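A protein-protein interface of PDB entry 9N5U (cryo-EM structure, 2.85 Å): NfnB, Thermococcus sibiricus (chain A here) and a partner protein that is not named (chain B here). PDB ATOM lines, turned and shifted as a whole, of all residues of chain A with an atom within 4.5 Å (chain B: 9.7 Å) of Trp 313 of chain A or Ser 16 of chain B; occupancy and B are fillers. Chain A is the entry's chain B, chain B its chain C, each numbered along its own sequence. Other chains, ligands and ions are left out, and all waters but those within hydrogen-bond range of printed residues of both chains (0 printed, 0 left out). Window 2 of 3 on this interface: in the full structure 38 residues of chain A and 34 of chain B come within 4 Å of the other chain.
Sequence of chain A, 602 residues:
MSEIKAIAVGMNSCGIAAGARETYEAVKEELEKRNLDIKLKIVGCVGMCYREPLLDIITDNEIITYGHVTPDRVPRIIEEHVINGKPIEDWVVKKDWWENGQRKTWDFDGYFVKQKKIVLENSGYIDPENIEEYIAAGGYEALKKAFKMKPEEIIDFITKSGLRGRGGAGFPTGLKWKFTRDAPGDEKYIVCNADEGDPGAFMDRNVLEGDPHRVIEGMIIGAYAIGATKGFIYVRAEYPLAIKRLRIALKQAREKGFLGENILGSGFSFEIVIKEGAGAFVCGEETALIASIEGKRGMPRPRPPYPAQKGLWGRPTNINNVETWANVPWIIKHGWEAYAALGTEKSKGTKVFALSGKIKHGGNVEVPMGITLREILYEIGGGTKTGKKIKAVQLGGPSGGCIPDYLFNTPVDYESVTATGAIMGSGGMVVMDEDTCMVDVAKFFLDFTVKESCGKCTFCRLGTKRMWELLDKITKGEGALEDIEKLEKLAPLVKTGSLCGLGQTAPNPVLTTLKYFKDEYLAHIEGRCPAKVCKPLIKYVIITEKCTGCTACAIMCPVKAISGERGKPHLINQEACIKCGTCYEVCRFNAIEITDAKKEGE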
ATOM      1  N   TYR A 189     -30.632  28.387  -6.822  1.00  0.00           N
ATOM      2  CA  TYR A 189     -29.227  28.736  -6.719  1.00  0.00           C
ATOM      3  C   TYR A 189     -28.465  28.138  -7.890  1.00  0.00           C
ATOM      4  O   TYR A 189     -28.892  27.160  -8.504  1.00  0.00           O
ATOM      5  CB  TYR A 189     -28.609  28.241  -5.407  1.00  0.00           C
ATOM      6  CG  TYR A 189     -29.367  28.633  -4.164  1.00  0.00           C
ATOM      7  CD1 TYR A 189     -29.313  29.925  -3.672  1.00  0.00           C
ATOM      8  CD2 TYR A 189     -30.122  27.702  -3.471  1.00  0.00           C
ATOM      9  CE1 TYR A 189     -29.996  30.282  -2.536  1.00  0.00           C
ATOM     10  CE2 TYR A 189     -30.806  28.050  -2.333  1.00  0.00           C
ATOM     11  CZ  TYR A 189     -30.740  29.341  -1.870  1.00  0.00           C
ATOM     12  OH  TYR A 189     -31.422  29.695  -0.733  1.00  0.00           O
ATOM     13  N   PHE A 232     -23.064  30.675  -6.045  1.00  0.00           N
ATOM     14  CA  PHE A 232     -21.965  30.260  -5.188  1.00  0.00           C
ATOM     15  C   PHE A 232     -20.785  29.848  -6.055  1.00  0.00           C
ATOM     16  O   PHE A 232     -20.940  29.045  -6.979  1.00  0.00           O
ATOM     17  CB  PHE A 232     -22.382  29.102  -4.275  1.00  0.00           C
ATOM     18  CG  PHE A 232     -23.510  29.435  -3.338  1.00  0.00           C
ATOM     19  CD1 PHE A 232     -23.256  29.985  -2.097  1.00  0.00           C
ATOM     20  CD2 PHE A 232     -24.823  29.188  -3.697  1.00  0.00           C
ATOM     21  CE1 PHE A 232     -24.289  30.288  -1.234  1.00  0.00           C
ATOM     22  CE2 PHE A 232     -25.859  29.489  -2.837  1.00  0.00           C
ATOM     23  CZ  PHE A 232     -25.592  30.040  -1.604  1.00  0.00           C
ATOM     24  N   ILE A 293     -21.471  22.763   1.384  1.00  0.00           N
ATOM     25  CA  ILE A 293     -21.950  24.138   1.499  1.00  0.00           C
ATOM     26  C   ILE A 293     -22.919  24.269   2.669  1.00  0.00           C
ATOM     27  O   ILE A 293     -22.941  25.294   3.360  1.00  0.00           O
ATOM     28  CB  ILE A 293     -22.583  24.599   0.172  1.00  0.00           C
ATOM     29  CG1 ILE A 293     -21.518  24.688  -0.920  1.00  0.00           C
ATOM     30  CG2 ILE A 293     -23.269  25.945   0.326  1.00  0.00           C
ATOM     31  CD1 ILE A 293     -22.054  25.137  -2.249  1.00  0.00           C
ATOM     32  N   GLU A 294     -23.710  23.230   2.929  1.00  0.00           N
ATOM     33  CA  GLU A 294     -24.692  23.224   4.005  1.00  0.00           C
ATOM     34  C   GLU A 294     -24.089  22.950   5.376  1.00  0.00           C
ATOM     35  O   GLU A 294     -24.832  22.929   6.362  1.00  0.00           O
ATOM     36  CB  GLU A 294     -25.778  22.189   3.717  1.00  0.00           C
ATOM     37  CG  GLU A 294     -26.684  22.543   2.564  1.00  0.00           C
ATOM     38  CD  GLU A 294     -27.719  21.476   2.300  1.00  0.00           C
ATOM     39  OE1 GLU A 294     -27.783  20.505   3.078  1.00  0.00           O
ATOM     40  OE2 GLU A 294     -28.467  21.606   1.313  1.00  0.00           O
ATOM     41  N   GLY A 295     -22.782  22.723   5.465  1.00  0.00           N
ATOM     42  CA  GLY A 295     -22.125  22.565   6.746  1.00  0.00           C
ATOM     43  C   GLY A 295     -22.023  21.153   7.272  1.00  0.00           C
ATOM     44  O   GLY A 295     -21.772  20.974   8.468  1.00  0.00           O
ATOM     45  N   GLY A 311     -31.522  20.515  -4.138  1.00  0.00           N
ATOM     46  CA  GLY A 311     -30.110  20.693  -3.867  1.00  0.00           C
ATOM     47  C   GLY A 311     -29.773  21.436  -2.591  1.00  0.00           C
ATOM     48  O   GLY A 311     -29.811  20.862  -1.500  1.00  0.00           O
ATOM     49  N   LEU A 312     -29.430  22.717  -2.719  1.00  0.00           N
ATOM     50  CA  LEU A 312     -28.944  23.515  -1.597  1.00  0.00           C
ATOM     51  C   LEU A 312     -30.108  23.923  -0.704  1.00  0.00           C
ATOM     52  O   LEU A 312     -30.956  24.727  -1.106  1.00  0.00           O
ATOM     53  CB  LEU A 312     -28.193  24.741  -2.102  1.00  0.00           C
ATOM     54  CG  LEU A 312     -26.701  24.535  -2.335  1.00  0.00           C
ATOM     55  CD1 LEU A 312     -26.049  25.817  -2.795  1.00  0.00           C
ATOM     56  CD2 LEU A 312     -26.064  24.032  -1.060  1.00  0.00           C
ATOM     57  N   TRP A 313     -30.131  23.377   0.513  1.00  0.00           N
ATOM     58  CA  TRP A 313     -31.192  23.602   1.496  1.00  0.00           C
ATOM     59  C   TRP A 313     -32.562  23.236   0.937  1.00  0.00           C
ATOM     60  O   TRP A 313     -33.575  23.835   1.299  1.00  0.00           O
ATOM     61  CB  TRP A 313     -31.180  25.043   2.018  1.00  0.00           C
ATOM     62  CG  TRP A 313     -29.915  25.396   2.740  1.00  0.00           C
ATOM     63  CD1 TRP A 313     -29.497  24.915   3.946  1.00  0.00           C
ATOM     64  CD2 TRP A 313     -28.902  26.305   2.301  1.00  0.00           C
ATOM     65  NE1 TRP A 313     -28.286  25.464   4.282  1.00  0.00           N
ATOM     66  CE2 TRP A 313     -27.899  26.321   3.287  1.00  0.00           C
ATOM     67  CE3 TRP A 313     -28.744  27.105   1.167  1.00  0.00           C
ATOM     68  CZ2 TRP A 313     -26.757  27.104   3.173  1.00  0.00           C
ATOM     69  CZ3 TRP A 313     -27.612  27.879   1.057  1.00  0.00           C
ATOM     70  CH2 TRP A 313     -26.632  27.875   2.053  1.00  0.00           C
ATOM     71  N   GLY A 314     -32.595  22.241   0.052  1.00  0.00           N
ATOM     72  CA  GLY A 314     -33.811  21.783  -0.570  1.00  0.00           C
ATOM     73  C   GLY A 314     -34.164  22.473  -1.869  1.00  0.00           C
ATOM     74  O   GLY A 314     -34.921  21.913  -2.666  1.00  0.00           O
ATOM     75  N   ARG A 315     -33.630  23.655  -2.110  1.00  0.00           N
ATOM     76  CA  ARG A 315     -33.985  24.408  -3.299  1.00  0.00           C
ATOM     77  C   ARG A 315     -33.178  23.936  -4.506  1.00  0.00           C
ATOM     78  O   ARG A 315     -32.062  23.436  -4.356  1.00  0.00           O
ATOM     79  CB  ARG A 315     -33.758  25.896  -3.069  1.00  0.00           C
ATOM     80  CG  ARG A 315     -34.953  26.599  -2.458  1.00  0.00           C
ATOM     81  CD  ARG A 315     -34.887  26.629  -0.951  1.00  0.00           C
ATOM     82  NE  ARG A 315     -33.894  27.581  -0.479  1.00  0.00           N
ATOM     83  CZ  ARG A 315     -33.798  27.999   0.774  1.00  0.00           C
ATOM     84  NH1 ARG A 315     -34.627  27.570   1.710  1.00  0.00           N
ATOM     85  NH2 ARG A 315     -32.848  28.872   1.095  1.00  0.00           N
ATOM     86  N   TYR B  11     -20.546  35.734  12.700  1.00  0.00           N
ATOM     87  CA  TYR B  11     -21.110  34.776  11.768  1.00  0.00           C
ATOM     88  C   TYR B  11     -22.564  34.483  12.109  1.00  0.00           C
ATOM     89  O   TYR B  11     -22.992  34.604  13.260  1.00  0.00           O
ATOM     90  CB  TYR B  11     -20.300  33.482  11.772  1.00  0.00           C
ATOM     91  CG  TYR B  11     -19.009  33.574  10.998  1.00  0.00           C
ATOM     92  CD1 TYR B  11     -18.975  33.307   9.639  1.00  0.00           C
ATOM     93  CD2 TYR B  11     -17.825  33.923  11.625  1.00  0.00           C
ATOM     94  CE1 TYR B  11     -17.803  33.388   8.927  1.00  0.00           C
ATOM     95  CE2 TYR B  11     -16.646  34.004  10.920  1.00  0.00           C
ATOM     96  CZ  TYR B  11     -16.641  33.736   9.572  1.00  0.00           C
ATOM     97  OH  TYR B  11     -15.466  33.817   8.864  1.00  0.00           O
ATOM     98  N   GLU B  12     -23.319  34.104  11.089  1.00  0.00           N
ATOM     99  CA  GLU B  12     -24.735  33.844  11.268  1.00  0.00           C
ATOM    100  C   GLU B  12     -24.936  32.552  12.057  1.00  0.00           C
ATOM    101  O   GLU B  12     -24.266  31.552  11.792  1.00  0.00           O
ATOM    102  CB  GLU B  12     -25.426  33.751   9.911  1.00  0.00           C
ATOM    103  CG  GLU B  12     -26.918  33.971   9.953  1.00  0.00           C
ATOM    104  CD  GLU B  12     -27.534  33.975   8.577  1.00  0.00           C
ATOM    105  OE1 GLU B  12     -26.886  33.472   7.638  1.00  0.00           O
ATOM    106  OE2 GLU B  12     -28.663  34.484   8.432  1.00  0.00           O
ATOM    107  N   PRO B  13     -25.853  32.539  13.035  1.00  0.00           N
ATOM    108  CA  PRO B  13     -26.119  31.336  13.835  1.00  0.00           C
ATOM    109  C   PRO B  13     -26.938  30.271  13.110  1.00  0.00           C
ATOM    110  O   PRO B  13     -27.913  29.743  13.644  1.00  0.00           O
ATOM    111  CB  PRO B  13     -26.871  31.897  15.044  1.00  0.00           C
ATOM    112  CG  PRO B  13     -27.554  33.092  14.521  1.00  0.00           C
ATOM    113  CD  PRO B  13     -26.601  33.702  13.538  1.00  0.00           C
ATOM    114  N   ASN B  14     -26.542  29.955  11.908  1.00  0.00           N
ATOM    115  CA  ASN B  14     -27.054  28.847  11.124  1.00  0.00           C
ATOM    116  C   ASN B  14     -26.029  27.723  11.086  1.00  0.00           C
ATOM    117  O   ASN B  14     -24.824  27.975  11.170  1.00  0.00           O
ATOM    118  CB  ASN B  14     -27.367  29.284   9.692  1.00  0.00           C
ATOM    119  CG  ASN B  14     -28.492  30.280   9.622  1.00  0.00           C
ATOM    120  OD1 ASN B  14     -29.292  30.395  10.549  1.00  0.00           O
ATOM    121  ND2 ASN B  14     -28.570  31.004   8.515  1.00  0.00           N
ATOM    122  N   PRO B  15     -26.469  26.470  10.971  1.00  0.00           N
ATOM    123  CA  PRO B  15     -25.506  25.361  10.895  1.00  0.00           C
ATOM    124  C   PRO B  15     -24.580  25.436   9.695  1.00  0.00           C
ATOM    125  O   PRO B  15     -23.495  24.848   9.734  1.00  0.00           O
ATOM    126  CB  PRO B  15     -26.406  24.120  10.831  1.00  0.00           C
ATOM    127  CG  PRO B  15     -27.674  24.550  11.465  1.00  0.00           C
ATOM    128  CD  PRO B  15     -27.855  25.986  11.086  1.00  0.00           C
ATOM    129  N   SER B  16     -24.975  26.142   8.634  1.00  0.00           N
ATOM    130  CA  SER B  16     -24.140  26.278   7.447  1.00  0.00           C
ATOM    131  C   SER B  16     -22.874  27.084   7.701  1.00  0.00           C
ATOM    132  O   SER B  16     -21.924  26.984   6.920  1.00  0.00           O
ATOM    133  CB  SER B  16     -24.941  26.929   6.324  1.00  0.00           C
ATOM    134  OG  SER B  16     -24.079  27.538   5.382  1.00  0.00           O
ATOM    135  N   SER B  17     -22.836  27.874   8.767  1.00  0.00           N
ATOM    136  CA  SER B  17     -21.675  28.697   9.062  1.00  0.00           C
ATOM    137  C   SER B  17     -20.554  27.919   9.738  1.00  0.00           C
ATOM    138  O   SER B  17     -19.528  28.515  10.067  1.00  0.00           O
ATOM    139  CB  SER B  17     -22.090  29.877   9.940  1.00  0.00           C
ATOM    140  OG  SER B  17     -21.018  30.784  10.103  1.00  0.00           O
ATOM    141  N   LEU B  18     -20.731  26.612   9.943  1.00  0.00           N
ATOM    142  CA  LEU B  18     -19.766  25.824  10.703  1.00  0.00           C
ATOM    143  C   LEU B  18     -18.407  25.771  10.014  1.00  0.00           C
ATOM    144  O   LEU B  18     -17.379  26.075  10.626  1.00  0.00           O
ATOM    145  CB  LEU B  18     -20.321  24.417  10.925  1.00  0.00           C
ATOM    146  CG  LEU B  18     -19.393  23.346  11.494  1.00  0.00           C
ATOM    147  CD1 LEU B  18     -18.838  23.764  12.841  1.00  0.00           C
ATOM    148  CD2 LEU B  18     -20.134  22.030  11.604  1.00  0.00           C
ATOM    149  N   ILE B  19     -18.379  25.382   8.743  1.00  0.00           N
ATOM    150  CA  ILE B  19     -17.120  25.236   8.012  1.00  0.00           C
ATOM    151  C   ILE B  19     -16.412  26.582   7.850  1.00  0.00           C
ATOM    152  O   ILE B  19     -15.194  26.643   8.076  1.00  0.00           O
ATOM    153  CB  ILE B  19     -17.337  24.531   6.662  1.00  0.00           C
ATOM    154  CG1 ILE B  19     -18.065  23.205   6.882  1.00  0.00           C
ATOM    155  CG2 ILE B  19     -16.008  24.273   5.981  1.00  0.00           C
ATOM    156  CD1 ILE B  19     -18.153  22.338   5.660  1.00  0.00           C
ATOM    157  N   PRO B  20     -17.092  27.679   7.471  1.00  0.00           N
ATOM    158  CA  PRO B  20     -16.408  28.986   7.526  1.00  0.00           C
ATOM    159  C   PRO B  20     -15.909  29.347   8.916  1.00  0.00           C
ATOM    160  O   PRO B  20     -14.835  29.944   9.050  1.00  0.00           O
ATOM    161  CB  PRO B  20     -17.483  29.962   7.035  1.00  0.00           C
ATOM    162  CG  PRO B  20     -18.356  29.151   6.178  1.00  0.00           C
ATOM    163  CD  PRO B  20     -18.412  27.806   6.822  1.00  0.00           C
ATOM    164  N   LEU B  21     -16.661  28.988   9.959  1.00  0.00           N
ATOM    165  CA  LEU B  21     -16.213  29.232  11.326  1.00  0.00           C
ATOM    166  C   LEU B  21     -14.998  28.383  11.678  1.00  0.00           C
ATOM    167  O   LEU B  21     -14.094  28.848  12.378  1.00  0.00           O
ATOM    168  CB  LEU B  21     -17.352  28.971  12.308  1.00  0.00           C
ATOM    169  CG  LEU B  21     -18.131  30.206  12.748  1.00  0.00           C
ATOM    170  CD1 LEU B  21     -19.424  29.814  13.427  1.00  0.00           C
ATOM    171  CD2 LEU B  21     -17.279  31.034  13.681  1.00  0.00           C
ATOM    172  N   LEU B  22     -14.959  27.134  11.211  1.00  0.00           N
ATOM    173  CA  LEU B  22     -13.784  26.300  11.443  1.00  0.00           C
ATOM    174  C   LEU B  22     -12.556  26.873  10.745  1.00  0.00           C
ATOM    175  O   LEU B  22     -11.453  26.868  11.306  1.00  0.00           O
ATOM    176  CB  LEU B  22     -14.057  24.871  10.979  1.00  0.00           C
ATOM    177  CG  LEU B  22     -15.079  24.082  11.799  1.00  0.00           C
ATOM    178  CD1 LEU B  22     -15.395  22.746  11.157  1.00  0.00           C
ATOM    179  CD2 LEU B  22     -14.569  23.883  13.204  1.00  0.00           C
ATOM    180  N   GLN B  23     -12.730  27.377   9.521  1.00  0.00           N
ATOM    181  CA  GLN B  23     -11.616  28.005   8.815  1.00  0.00           C
ATOM    182  C   GLN B  23     -11.150  29.272   9.525  1.00  0.00           C
ATOM    183  O   GLN B  23      -9.943  29.519   9.645  1.00  0.00           O
ATOM    184  CB  GLN B  23     -12.020  28.308   7.373  1.00  0.00           C
ATOM    185  CG  GLN B  23     -12.408  27.080   6.568  1.00  0.00           C
ATOM    186  CD  GLN B  23     -12.949  27.423   5.199  1.00  0.00           C
ATOM    187  OE1 GLN B  23     -13.178  28.588   4.884  1.00  0.00           O
ATOM    188  NE2 GLN B  23     -13.157  26.411   4.375  1.00  0.00           N
ATOM    189  N   ILE B  40     -18.524  27.187  19.393  1.00  0.00           N
ATOM    190  CA  ILE B  40     -19.124  27.090  18.064  1.00  0.00           C
ATOM    191  C   ILE B  40     -20.352  26.191  18.099  1.00  0.00           C
ATOM    192  O   ILE B  40     -21.388  26.505  17.502  1.00  0.00           O
ATOM    193  CB  ILE B  40     -18.081  26.589  17.046  1.00  0.00           C
ATOM    194  CG1 ILE B  40     -17.060  27.678  16.735  1.00  0.00           C
ATOM    195  CG2 ILE B  40     -18.744  26.135  15.762  1.00  0.00           C
ATOM    196  CD1 ILE B  40     -16.005  27.238  15.756  1.00  0.00           C
ATOM    197  N   TYR B  43     -23.105  28.205  19.882  1.00  0.00           N
ATOM    198  CA  TYR B  43     -23.656  29.327  19.129  1.00  0.00           C
ATOM    199  C   TYR B  43     -24.493  28.853  17.948  1.00  0.00           C
ATOM    200  O   TYR B  43     -25.568  29.400  17.684  1.00  0.00           O
ATOM    201  CB  TYR B  43     -22.524  30.236  18.657  1.00  0.00           C
ATOM    202  CG  TYR B  43     -22.973  31.430  17.849  1.00  0.00           C
ATOM    203  CD1 TYR B  43     -23.779  32.408  18.410  1.00  0.00           C
ATOM    204  CD2 TYR B  43     -22.576  31.586  16.532  1.00  0.00           C
ATOM    205  CE1 TYR B  43     -24.183  33.502  17.678  1.00  0.00           C
ATOM    206  CE2 TYR B  43     -22.974  32.677  15.795  1.00  0.00           C
ATOM    207  CZ  TYR B  43     -23.776  33.630  16.371  1.00  0.00           C
ATOM    208  OH  TYR B  43     -24.175  34.718  15.639  1.00  0.00           O
ATOM    209  N   LEU B  44     -24.013  27.850  17.220  1.00  0.00           N
ATOM    210  CA  LEU B  44     -24.741  27.341  16.068  1.00  0.00           C
ATOM    211  C   LEU B  44     -25.840  26.361  16.445  1.00  0.00           C
ATOM    212  O   LEU B  44     -26.666  26.032  15.589  1.00  0.00           O
ATOM    213  CB  LEU B  44     -23.775  26.668  15.095  1.00  0.00           C
ATOM    214  CG  LEU B  44     -22.637  27.545  14.581  1.00  0.00           C
ATOM    215  CD1 LEU B  44     -21.721  26.747  13.686  1.00  0.00           C
ATOM    216  CD2 LEU B  44     -23.185  28.748  13.849  1.00  0.00           C
ATOM    217  N   LYS B  45     -25.872  25.912  17.701  1.00  0.00           N
ATOM    218  CA  LYS B  45     -26.798  24.882  18.171  1.00  0.00           C
ATOM    219  C   LYS B  45     -26.683  23.610  17.331  1.00  0.00           C
ATOM    220  O   LYS B  45     -27.674  23.043  16.869  1.00  0.00           O
ATOM    221  CB  LYS B  45     -28.237  25.404  18.208  1.00  0.00           C
ATOM    222  CG  LYS B  45     -28.524  26.283  19.412  1.00  0.00           C
ATOM    223  CD  LYS B  45     -29.921  26.864  19.373  1.00  0.00           C
ATOM    224  CE  LYS B  45     -30.065  27.868  18.247  1.00  0.00           C
ATOM    225  NZ  LYS B  45     -31.434  28.446  18.195  1.00  0.00           N
ATOM    226  N   VAL B  46     -25.448  23.168  17.128  1.00  0.00           N
ATOM    227  CA  VAL B  46     -25.173  21.881  16.501  1.00  0.00           C
ATOM    228  C   VAL B  46     -24.496  20.998  17.542  1.00  0.00           C
ATOM    229  O   VAL B  46     -23.840  21.518  18.455  1.00  0.00           O
ATOM    230  CB  VAL B  46     -24.304  22.035  15.244  1.00  0.00           C
ATOM    231  CG1 VAL B  46     -25.092  22.697  14.133  1.00  0.00           C
ATOM    232  CG2 VAL B  46     -23.062  22.833  15.558  1.00  0.00           C
ATOM    233  N   VAL B  54     -17.264  16.912  11.166  1.00  0.00           N
ATOM    234  CA  VAL B  54     -16.923  17.814  10.070  1.00  0.00           C
ATOM    235  C   VAL B  54     -15.448  18.196  10.130  1.00  0.00           C
ATOM    236  O   VAL B  54     -14.755  18.203   9.107  1.00  0.00           O
ATOM    237  CB  VAL B  54     -17.838  19.051  10.089  1.00  0.00           C
ATOM    238  CG1 VAL B  54     -17.373  20.072   9.076  1.00  0.00           C
ATOM    239  CG2 VAL B  54     -19.266  18.646   9.799  1.00  0.00           C
ATOM    240  N   TYR B  58     -12.114  16.878   6.900  1.00  0.00           N
ATOM    241  CA  TYR B  58     -11.274  17.644   5.990  1.00  0.00           C
ATOM    242  C   TYR B  58      -9.833  17.661   6.478  1.00  0.00           C
ATOM    243  O   TYR B  58      -9.568  17.866   7.665  1.00  0.00           O
ATOM    244  CB  TYR B  58     -11.806  19.070   5.838  1.00  0.00           C
ATOM    245  CG  TYR B  58     -13.222  19.124   5.310  1.00  0.00           C
ATOM    246  CD1 TYR B  58     -13.481  19.068   3.948  1.00  0.00           C
ATOM    247  CD2 TYR B  58     -14.300  19.218   6.174  1.00  0.00           C
ATOM    248  CE1 TYR B  58     -14.769  19.114   3.467  1.00  0.00           C
ATOM    249  CE2 TYR B  58     -15.592  19.262   5.701  1.00  0.00           C
ATOM    250  CZ  TYR B  58     -15.820  19.211   4.347  1.00  0.00           C
ATOM    251  OH  TYR B  58     -17.105  19.257   3.873  1.00  0.00           O
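Ser 16 of chain B touches just these residues of chain A: Ile 293, Glu 294 and Trp 313. No residue of chain B comes within 4 Å of Gly 311 of chain A. No residue of chain B comes within 4 Å of Leu 312 of chain A. No residue of chain B comes within 4 Å of Gly 314 of chain A. Printed residues of chain B within 4 Å of Ile 293 of chain A: Ser 16 (3.2 Å). Printed residues of chain A within 4 Å of Val 54 of chain B: Gly 295 (3.7 Å). The nearest residue of chain B that does not touch Trp 313 of chain A is Pro 15 of chain B (6.6 Å). The nearest printed residue of chain B that does not touch Gly 295 of chain A is Pro 15 of chain B (4.002 Å).
Of the 10 printed residues of chain A, 4 touch a printed residue of chain B. Printed residues of chain A that touch a printed residue of chain B: Ile 293, Glu 294, Gly 295 and Trp 313. Of the 20 printed residues of chain B, 3 touch a printed residue of chain A. Hydrophobic or aromatic side chains of chain B that line the printed part of chain A: Leu 18 and Val 54. Among the printed residues, 5 pairs touch across the chains.
N of Trp 313 of chain A lies within hydrogen-bond range of OE2 of Glu 294 of chain A.
The backbone carbonyl oxygen (O) of Ile 293 of chain A lies within hydrogen-bond range of the side-chain hydroxyl (OG) of Ser 16 of chain B, 3.2 Å away.
Among the printed residues, pairs that only touch across the chains: Trp 313 of chain A with Ser 16 of chain B (3.5 Å), Glu 294 of chain A with Ser 16 of chain B (3.6 Å), Gly 295 of chain A with Val 54 of chain B (3.7 Å) and Gly 295 of chain A with Leu 18 of chain B (3.7 Å).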
